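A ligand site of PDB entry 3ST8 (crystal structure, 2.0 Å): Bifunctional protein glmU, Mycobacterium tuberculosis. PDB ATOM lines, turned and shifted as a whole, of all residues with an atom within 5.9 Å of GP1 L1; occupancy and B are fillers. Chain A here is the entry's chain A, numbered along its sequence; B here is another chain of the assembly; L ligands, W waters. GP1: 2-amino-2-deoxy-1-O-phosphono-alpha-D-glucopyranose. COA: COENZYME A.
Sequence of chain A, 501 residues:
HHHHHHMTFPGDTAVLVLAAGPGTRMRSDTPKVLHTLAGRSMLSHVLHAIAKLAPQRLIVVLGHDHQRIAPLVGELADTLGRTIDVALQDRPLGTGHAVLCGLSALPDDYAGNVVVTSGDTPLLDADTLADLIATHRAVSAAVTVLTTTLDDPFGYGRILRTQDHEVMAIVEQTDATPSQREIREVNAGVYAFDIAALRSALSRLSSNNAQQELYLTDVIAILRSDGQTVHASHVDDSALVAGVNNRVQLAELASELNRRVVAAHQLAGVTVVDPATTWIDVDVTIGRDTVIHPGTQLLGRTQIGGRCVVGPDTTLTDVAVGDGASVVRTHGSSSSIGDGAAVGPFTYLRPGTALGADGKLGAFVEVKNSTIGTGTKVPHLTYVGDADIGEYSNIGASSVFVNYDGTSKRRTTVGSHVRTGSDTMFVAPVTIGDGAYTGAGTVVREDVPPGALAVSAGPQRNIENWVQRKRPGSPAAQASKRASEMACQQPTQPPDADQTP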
ATOM      1  N   ARG A 350      22.849   4.700  20.270  1.00  0.00           N
ATOM      2  CA  ARG A 350      23.945   4.407  19.349  1.00  0.00           C
ATOM      3  C   ARG A 350      24.835   3.396  20.078  1.00  0.00           C
ATOM      4  O   ARG A 350      24.685   3.216  21.287  1.00  0.00           O
ATOM      5  CB  ARG A 350      24.690   5.691  19.036  1.00  0.00           C
ATOM      6  CG  ARG A 350      23.779   6.512  18.024  1.00  0.00           C
ATOM      7  CD  ARG A 350      24.315   7.940  17.755  1.00  0.00           C
ATOM      8  NE  ARG A 350      25.679   7.964  17.223  1.00  0.00           N
ATOM      9  CZ  ARG A 350      26.527   8.945  17.479  1.00  0.00           C
ATOM     10  NH1 ARG A 350      26.159   9.980  18.273  1.00  0.00           N
ATOM     11  NH2 ARG A 350      27.809   8.900  17.003  1.00  0.00           N
ATOM     12  N   GLU A 366      19.249  11.097  23.037  1.00  0.00           N
ATOM     13  CA  GLU A 366      20.166  10.334  22.191  1.00  0.00           C
ATOM     14  C   GLU A 366      21.339   9.953  23.136  1.00  0.00           C
ATOM     15  O   GLU A 366      21.869  10.834  23.856  1.00  0.00           O
ATOM     16  CB  GLU A 366      20.743  11.183  21.047  1.00  0.00           C
ATOM     17  CG  GLU A 366      21.940  10.491  20.337  1.00  0.00           C
ATOM     18  CD  GLU A 366      22.449  11.245  19.094  1.00  0.00           C
ATOM     19  OE1 GLU A 366      21.723  12.143  18.558  1.00  0.00           O
ATOM     20  OE2 GLU A 366      23.616  10.960  18.659  1.00  0.00           O
ATOM     21  N   LYS A 368      25.160   7.732  23.171  1.00  0.00           N
ATOM     22  CA  LYS A 368      26.191   7.074  22.387  1.00  0.00           C
ATOM     23  C   LYS A 368      27.290   6.667  23.398  1.00  0.00           C
ATOM     24  O   LYS A 368      27.742   7.551  24.168  1.00  0.00           O
ATOM     25  CB  LYS A 368      26.756   8.162  21.385  1.00  0.00           C
ATOM     26  CG  LYS A 368      28.058   7.703  20.555  1.00  0.00           C
ATOM     27  CD  LYS A 368      29.253   8.681  20.951  1.00  0.00           C
ATOM     28  CE  LYS A 368      30.520   8.298  20.245  1.00  0.00           C
ATOM     29  NZ  LYS A 368      31.451   9.482  20.384  1.00  0.00           N
ATOM     30  N   TYR A 383      21.336  14.952  25.103  1.00  0.00           N
ATOM     31  CA  TYR A 383      22.317  14.085  24.410  1.00  0.00           C
ATOM     32  C   TYR A 383      23.394  13.634  25.466  1.00  0.00           C
ATOM     33  O   TYR A 383      23.927  14.445  26.187  1.00  0.00           O
ATOM     34  CB  TYR A 383      23.056  14.971  23.341  1.00  0.00           C
ATOM     35  CG  TYR A 383      24.326  14.253  22.841  1.00  0.00           C
ATOM     36  CD1 TYR A 383      24.244  13.300  21.866  1.00  0.00           C
ATOM     37  CD2 TYR A 383      25.605  14.640  23.322  1.00  0.00           C
ATOM     38  CE1 TYR A 383      25.448  12.571  21.425  1.00  0.00           C
ATOM     39  CE2 TYR A 383      26.762  13.993  22.884  1.00  0.00           C
ATOM     40  CZ  TYR A 383      26.683  12.983  21.950  1.00  0.00           C
ATOM     41  OH  TYR A 383      27.832  12.308  21.501  1.00  0.00           O
ATOM     42  N   GLY A 385      26.889  11.515  25.457  1.00  0.00           N
ATOM     43  CA  GLY A 385      27.889  10.849  24.573  1.00  0.00           C
ATOM     44  C   GLY A 385      29.144  10.708  25.430  1.00  0.00           C
ATOM     45  O   GLY A 385      29.475  11.620  26.171  1.00  0.00           O
ATOM     46  N   ASP A 386      29.748   9.530  25.426  1.00  0.00           N
ATOM     47  CA  ASP A 386      31.083   9.240  26.046  1.00  0.00           C
ATOM     48  C   ASP A 386      31.010   9.514  27.580  1.00  0.00           C
ATOM     49  O   ASP A 386      31.897  10.175  28.146  1.00  0.00           O
ATOM     50  CB  ASP A 386      32.159  10.028  25.325  1.00  0.00           C
ATOM     51  CG  ASP A 386      32.347   9.555  23.876  1.00  0.00           C
ATOM     52  OD1 ASP A 386      32.654   8.376  23.751  1.00  0.00           O
ATOM     53  OD2 ASP A 386      32.156  10.330  22.917  1.00  0.00           O
ATOM     54  N   PHE A 401      25.904  16.325  27.256  1.00  0.00           N
ATOM     55  CA  PHE A 401      27.271  15.911  27.606  1.00  0.00           C
ATOM     56  C   PHE A 401      28.152  16.331  26.424  1.00  0.00           C
ATOM     57  O   PHE A 401      28.133  15.715  25.377  1.00  0.00           O
ATOM     58  CB  PHE A 401      27.266  14.421  27.828  1.00  0.00           C
ATOM     59  CG  PHE A 401      26.629  14.071  29.141  1.00  0.00           C
ATOM     60  CD1 PHE A 401      27.456  13.832  30.261  1.00  0.00           C
ATOM     61  CD2 PHE A 401      25.222  14.082  29.340  1.00  0.00           C
ATOM     62  CE1 PHE A 401      26.882  13.542  31.568  1.00  0.00           C
ATOM     63  CE2 PHE A 401      24.601  13.704  30.638  1.00  0.00           C
ATOM     64  CZ  PHE A 401      25.435  13.501  31.781  1.00  0.00           C
ATOM     65  N   ASN A 403      30.849  16.428  24.373  1.00  0.00           N
ATOM     66  CA  ASN A 403      31.990  15.515  24.362  1.00  0.00           C
ATOM     67  C   ASN A 403      32.993  15.864  23.209  1.00  0.00           C
ATOM     68  O   ASN A 403      33.760  15.018  22.868  1.00  0.00           O
ATOM     69  CB  ASN A 403      31.461  14.099  24.124  1.00  0.00           C
ATOM     70  CG  ASN A 403      30.797  13.932  22.663  1.00  0.00           C
ATOM     71  OD1 ASN A 403      30.326  14.902  22.043  1.00  0.00           O
ATOM     72  ND2 ASN A 403      30.830  12.691  22.143  1.00  0.00           N
ATOM     73  N   TYR A 404      32.918  17.055  22.598  1.00  0.00           N
ATOM     74  CA  TYR A 404      33.743  17.330  21.379  1.00  0.00           C
ATOM     75  C   TYR A 404      34.286  18.691  21.544  1.00  0.00           C
ATOM     76  O   TYR A 404      33.519  19.703  21.562  1.00  0.00           O
ATOM     77  CB  TYR A 404      32.816  17.352  20.149  1.00  0.00           C
ATOM     78  CG  TYR A 404      33.433  17.673  18.816  1.00  0.00           C
ATOM     79  CD1 TYR A 404      34.545  16.939  18.328  1.00  0.00           C
ATOM     80  CD2 TYR A 404      32.810  18.629  17.938  1.00  0.00           C
ATOM     81  CE1 TYR A 404      35.073  17.163  17.042  1.00  0.00           C
ATOM     82  CE2 TYR A 404      33.350  18.862  16.608  1.00  0.00           C
ATOM     83  CZ  TYR A 404      34.471  18.149  16.200  1.00  0.00           C
ATOM     84  OH  TYR A 404      34.977  18.308  14.930  1.00  0.00           O
ATOM     85  N   LYS A 409      37.334  13.853  21.003  1.00  0.00           N
ATOM     86  CA  LYS A 409      36.197  13.477  21.898  1.00  0.00           C
ATOM     87  C   LYS A 409      36.698  13.345  23.309  1.00  0.00           C
ATOM     88  O   LYS A 409      37.793  12.768  23.510  1.00  0.00           O
ATOM     89  CB  LYS A 409      35.514  12.202  21.478  1.00  0.00           C
ATOM     90  CG  LYS A 409      35.142  12.088  19.926  1.00  0.00           C
ATOM     91  CD  LYS A 409      34.106  13.173  19.507  1.00  0.00           C
ATOM     92  CE  LYS A 409      33.822  13.148  17.962  1.00  0.00           C
ATOM     93  NZ  LYS A 409      32.863  12.041  17.634  1.00  0.00           N
ATOM     94  N   LYS B 377      27.533  19.729   9.708  1.00  0.00           N
ATOM     95  CA  LYS B 377      26.783  18.781  10.538  1.00  0.00           C
ATOM     96  C   LYS B 377      25.991  19.557  11.548  1.00  0.00           C
ATOM     97  O   LYS B 377      26.518  20.488  12.157  1.00  0.00           O
ATOM     98  CB  LYS B 377      27.773  17.853  11.271  1.00  0.00           C
ATOM     99  CG  LYS B 377      28.516  16.990  10.153  1.00  0.00           C
ATOM    100  CD  LYS B 377      29.358  15.971  10.738  1.00  0.00           C
ATOM    101  CE  LYS B 377      30.138  15.323   9.530  1.00  0.00           C
ATOM    102  NZ  LYS B 377      30.912  14.312  10.369  1.00  0.00           N
ATOM    103  N   PRO B 379      24.180  17.952  14.376  1.00  0.00           N
ATOM    104  CA  PRO B 379      23.927  16.611  14.674  1.00  0.00           C
ATOM    105  C   PRO B 379      22.800  16.362  15.755  1.00  0.00           C
ATOM    106  O   PRO B 379      22.265  15.205  15.805  1.00  0.00           O
ATOM    107  CB  PRO B 379      25.289  16.110  15.236  1.00  0.00           C
ATOM    108  CG  PRO B 379      25.864  17.341  15.842  1.00  0.00           C
ATOM    109  CD  PRO B 379      25.555  18.332  14.699  1.00  0.00           C
ATOM    110  N   HIS B 380      22.451  17.356  16.593  1.00  0.00           N
ATOM    111  CA  HIS B 380      21.543  16.991  17.739  1.00  0.00           C
ATOM    112  C   HIS B 380      20.679  18.128  18.186  1.00  0.00           C
ATOM    113  O   HIS B 380      21.171  19.209  18.549  1.00  0.00           O
ATOM    114  CB  HIS B 380      22.384  16.659  19.063  1.00  0.00           C
ATOM    115  CG  HIS B 380      23.661  15.827  18.826  1.00  0.00           C
ATOM    116  ND1 HIS B 380      23.626  14.460  18.595  1.00  0.00           N
ATOM    117  CD2 HIS B 380      24.986  16.163  18.876  1.00  0.00           C
ATOM    118  CE1 HIS B 380      24.868  13.999  18.487  1.00  0.00           C
ATOM    119  NE2 HIS B 380      25.700  15.015  18.687  1.00  0.00           N
ATOM    120  N   ASN B 394      30.347  22.772  12.162  1.00  0.00           N
ATOM    121  CA  ASN B 394      29.646  21.875  13.071  1.00  0.00           C
ATOM    122  C   ASN B 394      28.838  22.764  14.031  1.00  0.00           C
ATOM    123  O   ASN B 394      29.371  23.760  14.580  1.00  0.00           O
ATOM    124  CB  ASN B 394      30.684  21.126  13.960  1.00  0.00           C
ATOM    125  CG  ASN B 394      30.037  19.965  14.724  1.00  0.00           C
ATOM    126  OD1 ASN B 394      29.687  18.938  14.070  1.00  0.00           O
ATOM    127  ND2 ASN B 394      29.778  20.117  16.029  1.00  0.00           N
ATOM    128  N   ILE B 395      27.536  22.506  14.105  1.00  0.00           N
ATOM    129  CA  ILE B 395      26.670  23.279  15.029  1.00  0.00           C
ATOM    130  C   ILE B 395      26.429  22.398  16.287  1.00  0.00           C
ATOM    131  O   ILE B 395      25.909  21.258  16.158  1.00  0.00           O
ATOM    132  CB  ILE B 395      25.250  23.544  14.325  1.00  0.00           C
ATOM    133  CG1 ILE B 395      25.474  24.290  13.001  1.00  0.00           C
ATOM    134  CG2 ILE B 395      24.414  24.389  15.296  1.00  0.00           C
ATOM    135  CD1 ILE B 395      26.341  25.640  13.158  1.00  0.00           C
ATOM    136  N   GLY B 396      26.768  22.904  17.455  1.00  0.00           N
ATOM    137  CA  GLY B 396      26.769  22.066  18.644  1.00  0.00           C
ATOM    138  C   GLY B 396      25.351  21.699  19.046  1.00  0.00           C
ATOM    139  O   GLY B 396      24.379  22.356  18.633  1.00  0.00           O
ATOM    140  N   ALA B 397      25.253  20.625  19.831  1.00  0.00           N
ATOM    141  CA  ALA B 397      23.956  20.067  20.240  1.00  0.00           C
ATOM    142  C   ALA B 397      23.104  21.119  20.902  1.00  0.00           C
ATOM    143  O   ALA B 397      23.597  21.934  21.653  1.00  0.00           O
ATOM    144  CB  ALA B 397      24.180  18.960  21.252  1.00  0.00           C
HETATM  145  C1  GP1 L   1      30.081  14.596  18.625  1.00  0.00           C
HETATM  146  C2  GP1 L   1      29.498  15.999  18.859  1.00  0.00           C
HETATM  147  C3  GP1 L   1      28.927  16.580  17.520  1.00  0.00           C
HETATM  148  C4  GP1 L   1      29.864  16.359  16.282  1.00  0.00           C
HETATM  149  C5  GP1 L   1      30.697  15.004  16.223  1.00  0.00           C
HETATM  150  C6  GP1 L   1      31.860  14.958  15.159  1.00  0.00           C
HETATM  151  N2  GP1 L   1      28.531  15.808  19.987  1.00  0.00           N
HETATM  152  O1  GP1 L   1      28.993  13.709  18.255  1.00  0.00           O
HETATM  153  O3  GP1 L   1      28.760  18.028  17.700  1.00  0.00           O
HETATM  154  O4  GP1 L   1      29.186  16.536  15.051  1.00  0.00           O
HETATM  155  O6  GP1 L   1      32.340  13.583  15.120  1.00  0.00           O
HETATM  156  O5  GP1 L   1      31.136  14.607  17.599  1.00  0.00           O
HETATM  157  O7B GP1 L   1      28.026  11.480  19.241  1.00  0.00           O
HETATM  158  P4B GP1 L   1      29.256  12.073  18.421  1.00  0.00           P
HETATM  159  O8B GP1 L   1      30.671  11.828  19.079  1.00  0.00           O
HETATM  160  O9B GP1 L   1      29.214  11.437  17.045  1.00  0.00           O
HETATM  161  N1A COA L   2      31.160  29.863  28.509  1.00  0.00           N
HETATM  162  C2A COA L   2      31.627  30.983  29.059  1.00  0.00           C
HETATM  163  N3A COA L   2      32.921  31.260  29.144  1.00  0.00           N
HETATM  164  C4A COA L   2      33.800  30.336  28.712  1.00  0.00           C
HETATM  165  C5A COA L   2      33.354  29.160  28.164  1.00  0.00           C
HETATM  166  C6A COA L   2      31.969  28.920  28.048  1.00  0.00           C
HETATM  167  N6A COA L   2      31.507  27.773  27.474  1.00  0.00           N
HETATM  168  N7A COA L   2      34.439  28.438  27.804  1.00  0.00           N
HETATM  169  C8A COA L   2      35.550  29.228  28.052  1.00  0.00           C
HETATM  170  N9A COA L   2      35.133  30.355  28.638  1.00  0.00           N
HETATM  171  C1B COA L   2      35.963  31.517  29.026  1.00  0.00           C
HETATM  172  C2B COA L   2      37.143  31.025  29.887  1.00  0.00           C
HETATM  173  O2B COA L   2      36.635  31.389  31.173  1.00  0.00           O
HETATM  174  C3B COA L   2      38.286  31.957  29.394  1.00  0.00           C
HETATM  175  O3B COA L   2      37.994  33.275  29.862  1.00  0.00           O
HETATM  176  P3B COA L   2      38.994  34.031  30.989  1.00  0.00           P
HETATM  177  O7A COA L   2      40.306  33.927  30.191  1.00  0.00           O
HETATM  178  O8A COA L   2      38.219  35.323  31.407  1.00  0.00           O
HETATM  179  O9A COA L   2      38.893  33.179  32.273  1.00  0.00           O
HETATM  180  C4B COA L   2      38.067  32.126  27.925  1.00  0.00           C
HETATM  181  O4B COA L   2      36.621  31.749  27.727  1.00  0.00           O
HETATM  182  C5B COA L   2      39.135  31.321  27.181  1.00  0.00           C
HETATM  183  O5B COA L   2      38.670  30.052  27.571  1.00  0.00           O
HETATM  184  P1A COA L   2      39.864  29.035  27.743  1.00  0.00           P
HETATM  185  O1A COA L   2      40.845  29.095  28.822  1.00  0.00           O
HETATM  186  O2A COA L   2      40.624  29.604  26.536  1.00  0.00           O
HETATM  187  O3A COA L   2      39.283  27.521  27.797  1.00  0.00           O
HETATM  188  P2A COA L   2      39.613  26.771  26.439  1.00  0.00           P
HETATM  189  O4A COA L   2      40.134  25.376  26.592  1.00  0.00           O
HETATM  190  O5A COA L   2      40.503  27.769  25.747  1.00  0.00           O
HETATM  191  O6A COA L   2      38.189  26.648  25.667  1.00  0.00           O
HETATM  192  CBP COA L   2      36.059  25.816  25.211  1.00  0.00           C
HETATM  193  CCP COA L   2      37.200  25.915  26.265  1.00  0.00           C
HETATM  194  CDP COA L   2      35.499  27.127  24.736  1.00  0.00           C
HETATM  195  CEP COA L   2      36.524  24.966  24.033  1.00  0.00           C
HETATM  196  CAP COA L   2      35.053  25.045  26.041  1.00  0.00           C
HETATM  197  OAP COA L   2      34.843  25.738  27.330  1.00  0.00           O
HETATM  198  C9P COA L   2      33.677  24.944  25.372  1.00  0.00           C
HETATM  199  O9P COA L   2      32.826  25.808  25.646  1.00  0.00           O
HETATM  200  N8P COA L   2      33.481  23.848  24.612  1.00  0.00           N
HETATM  201  C7P COA L   2      32.226  23.571  23.867  1.00  0.00           C
HETATM  202  C6P COA L   2      32.481  22.496  22.835  1.00  0.00           C
HETATM  203  C5P COA L   2      31.095  22.146  22.280  1.00  0.00           C
HETATM  204  O5P COA L   2      30.052  22.664  22.779  1.00  0.00           O
HETATM  205  N4P COA L   2      30.999  21.263  21.295  1.00  0.00           N
HETATM  206  C3P COA L   2      29.759  20.781  20.636  1.00  0.00           C
HETATM  207  C2P COA L   2      29.328  19.441  21.320  1.00  0.00           C
HETATM  208  S1P COA L   2      27.798  18.823  20.468  1.00  0.00           S
HETATM  209  O   HOH W   1      35.145  14.142  14.499  1.00  0.00           O
HETATM  210  O   HOH W   2      31.028  10.296  15.651  1.00  0.00           O
HETATM  211  O   HOH W   3      34.451  11.371  15.200  1.00  0.00           O
HETATM  212  O   HOH W   4      27.977  14.438  13.862  1.00  0.00           O
HETATM  213  O   HOH W   5      27.130  12.267  15.371  1.00  0.00           O
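N of Ala 397 of chain B lies close to S1P of COA L2 (3.2 Å). NH1 of Arg 350 is in salt-bridge range of O7B of GP1 L1, 2.6 Å away. An oxygen (O8B) of GP1 L1 lies within salt-bridge range of the side-chain amino group (NZ) of Lys 409 (2.6 Å). An oxygen (O7B) of GP1 L1 lies within hydrogen-bond range of the side-chain hydroxyl (OH) of Tyr 383 (2.4 Å). NE2 of His 380 of chain B is in hydrogen-bond range of N2 of GP1 L1 (3.2 Å). The side-chain amino group (NZ) of Lys 368 lies within salt-bridge range of an oxygen (O8B) of GP1 L1, 2.8 Å away. The backbone carbonyl oxygen of Tyr 404 sits at hydrogen-bond distance from a nitrogen (N4P) of COA L2, 3.0 Å away. A nitrogen (N2) of GP1 L1 sits at hydrogen-bond distance from the side-chain amide oxygen (OD1) of Asn 403 (2.9 Å). The side-chain amide oxygen (OD1) of Asn 394 of chain B lies within hydrogen-bond range of an oxygen (O4) of GP1 L1, at 2.6 Å.
An oxygen (O3) of GP1 L1 sits close to a sulfur (S1P) of COA L2, 3.0 Å away.
The backbone carbonyl oxygen of Tyr 383 lies within hydrogen-bond range of the backbone NH of Phe 401. A ring nitrogen (ND1) of His 380 of chain B sits at hydrogen-bond distance from the side-chain carboxylate (OE1) of Glu 366 (3.0 Å). The side-chain carboxylate (OE2) of Glu 366 lies within salt-bridge range of the guanidinium group (NH1) of Arg 350, 2.8 Å away. OH of Tyr 383 is in hydrogen-bond range of ND2 of Asn 403, at 3.1 Å. ND2 of Asn 403 is in hydrogen-bond range of OD2 of Asp 386 (2.8 Å). NZ of Lys 368 lies within salt-bridge range of OD2 of Asp 386, at 2.8 Å.
Residues that only touch GP1 L1: Pro 379 of chain B (3.5 Å) and Tyr 404 (3.8 Å). Nine residues have an atom within 4 Å of GP1 L1: Arg 350, Lys 368, Tyr 383, Asn 403, Tyr 404, Lys 409, Pro 379 of chain B, His 380 of chain B and Asn 394 of chain B.
Water W2 lies within hydrogen-bond range of O9B of GP1 L1 and NZ of Lys 409. Water W3 lies within hydrogen-bond range of NZ of Lys 409 (3.0 Å) and O6 of GP1 L1 (3.1 Å).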
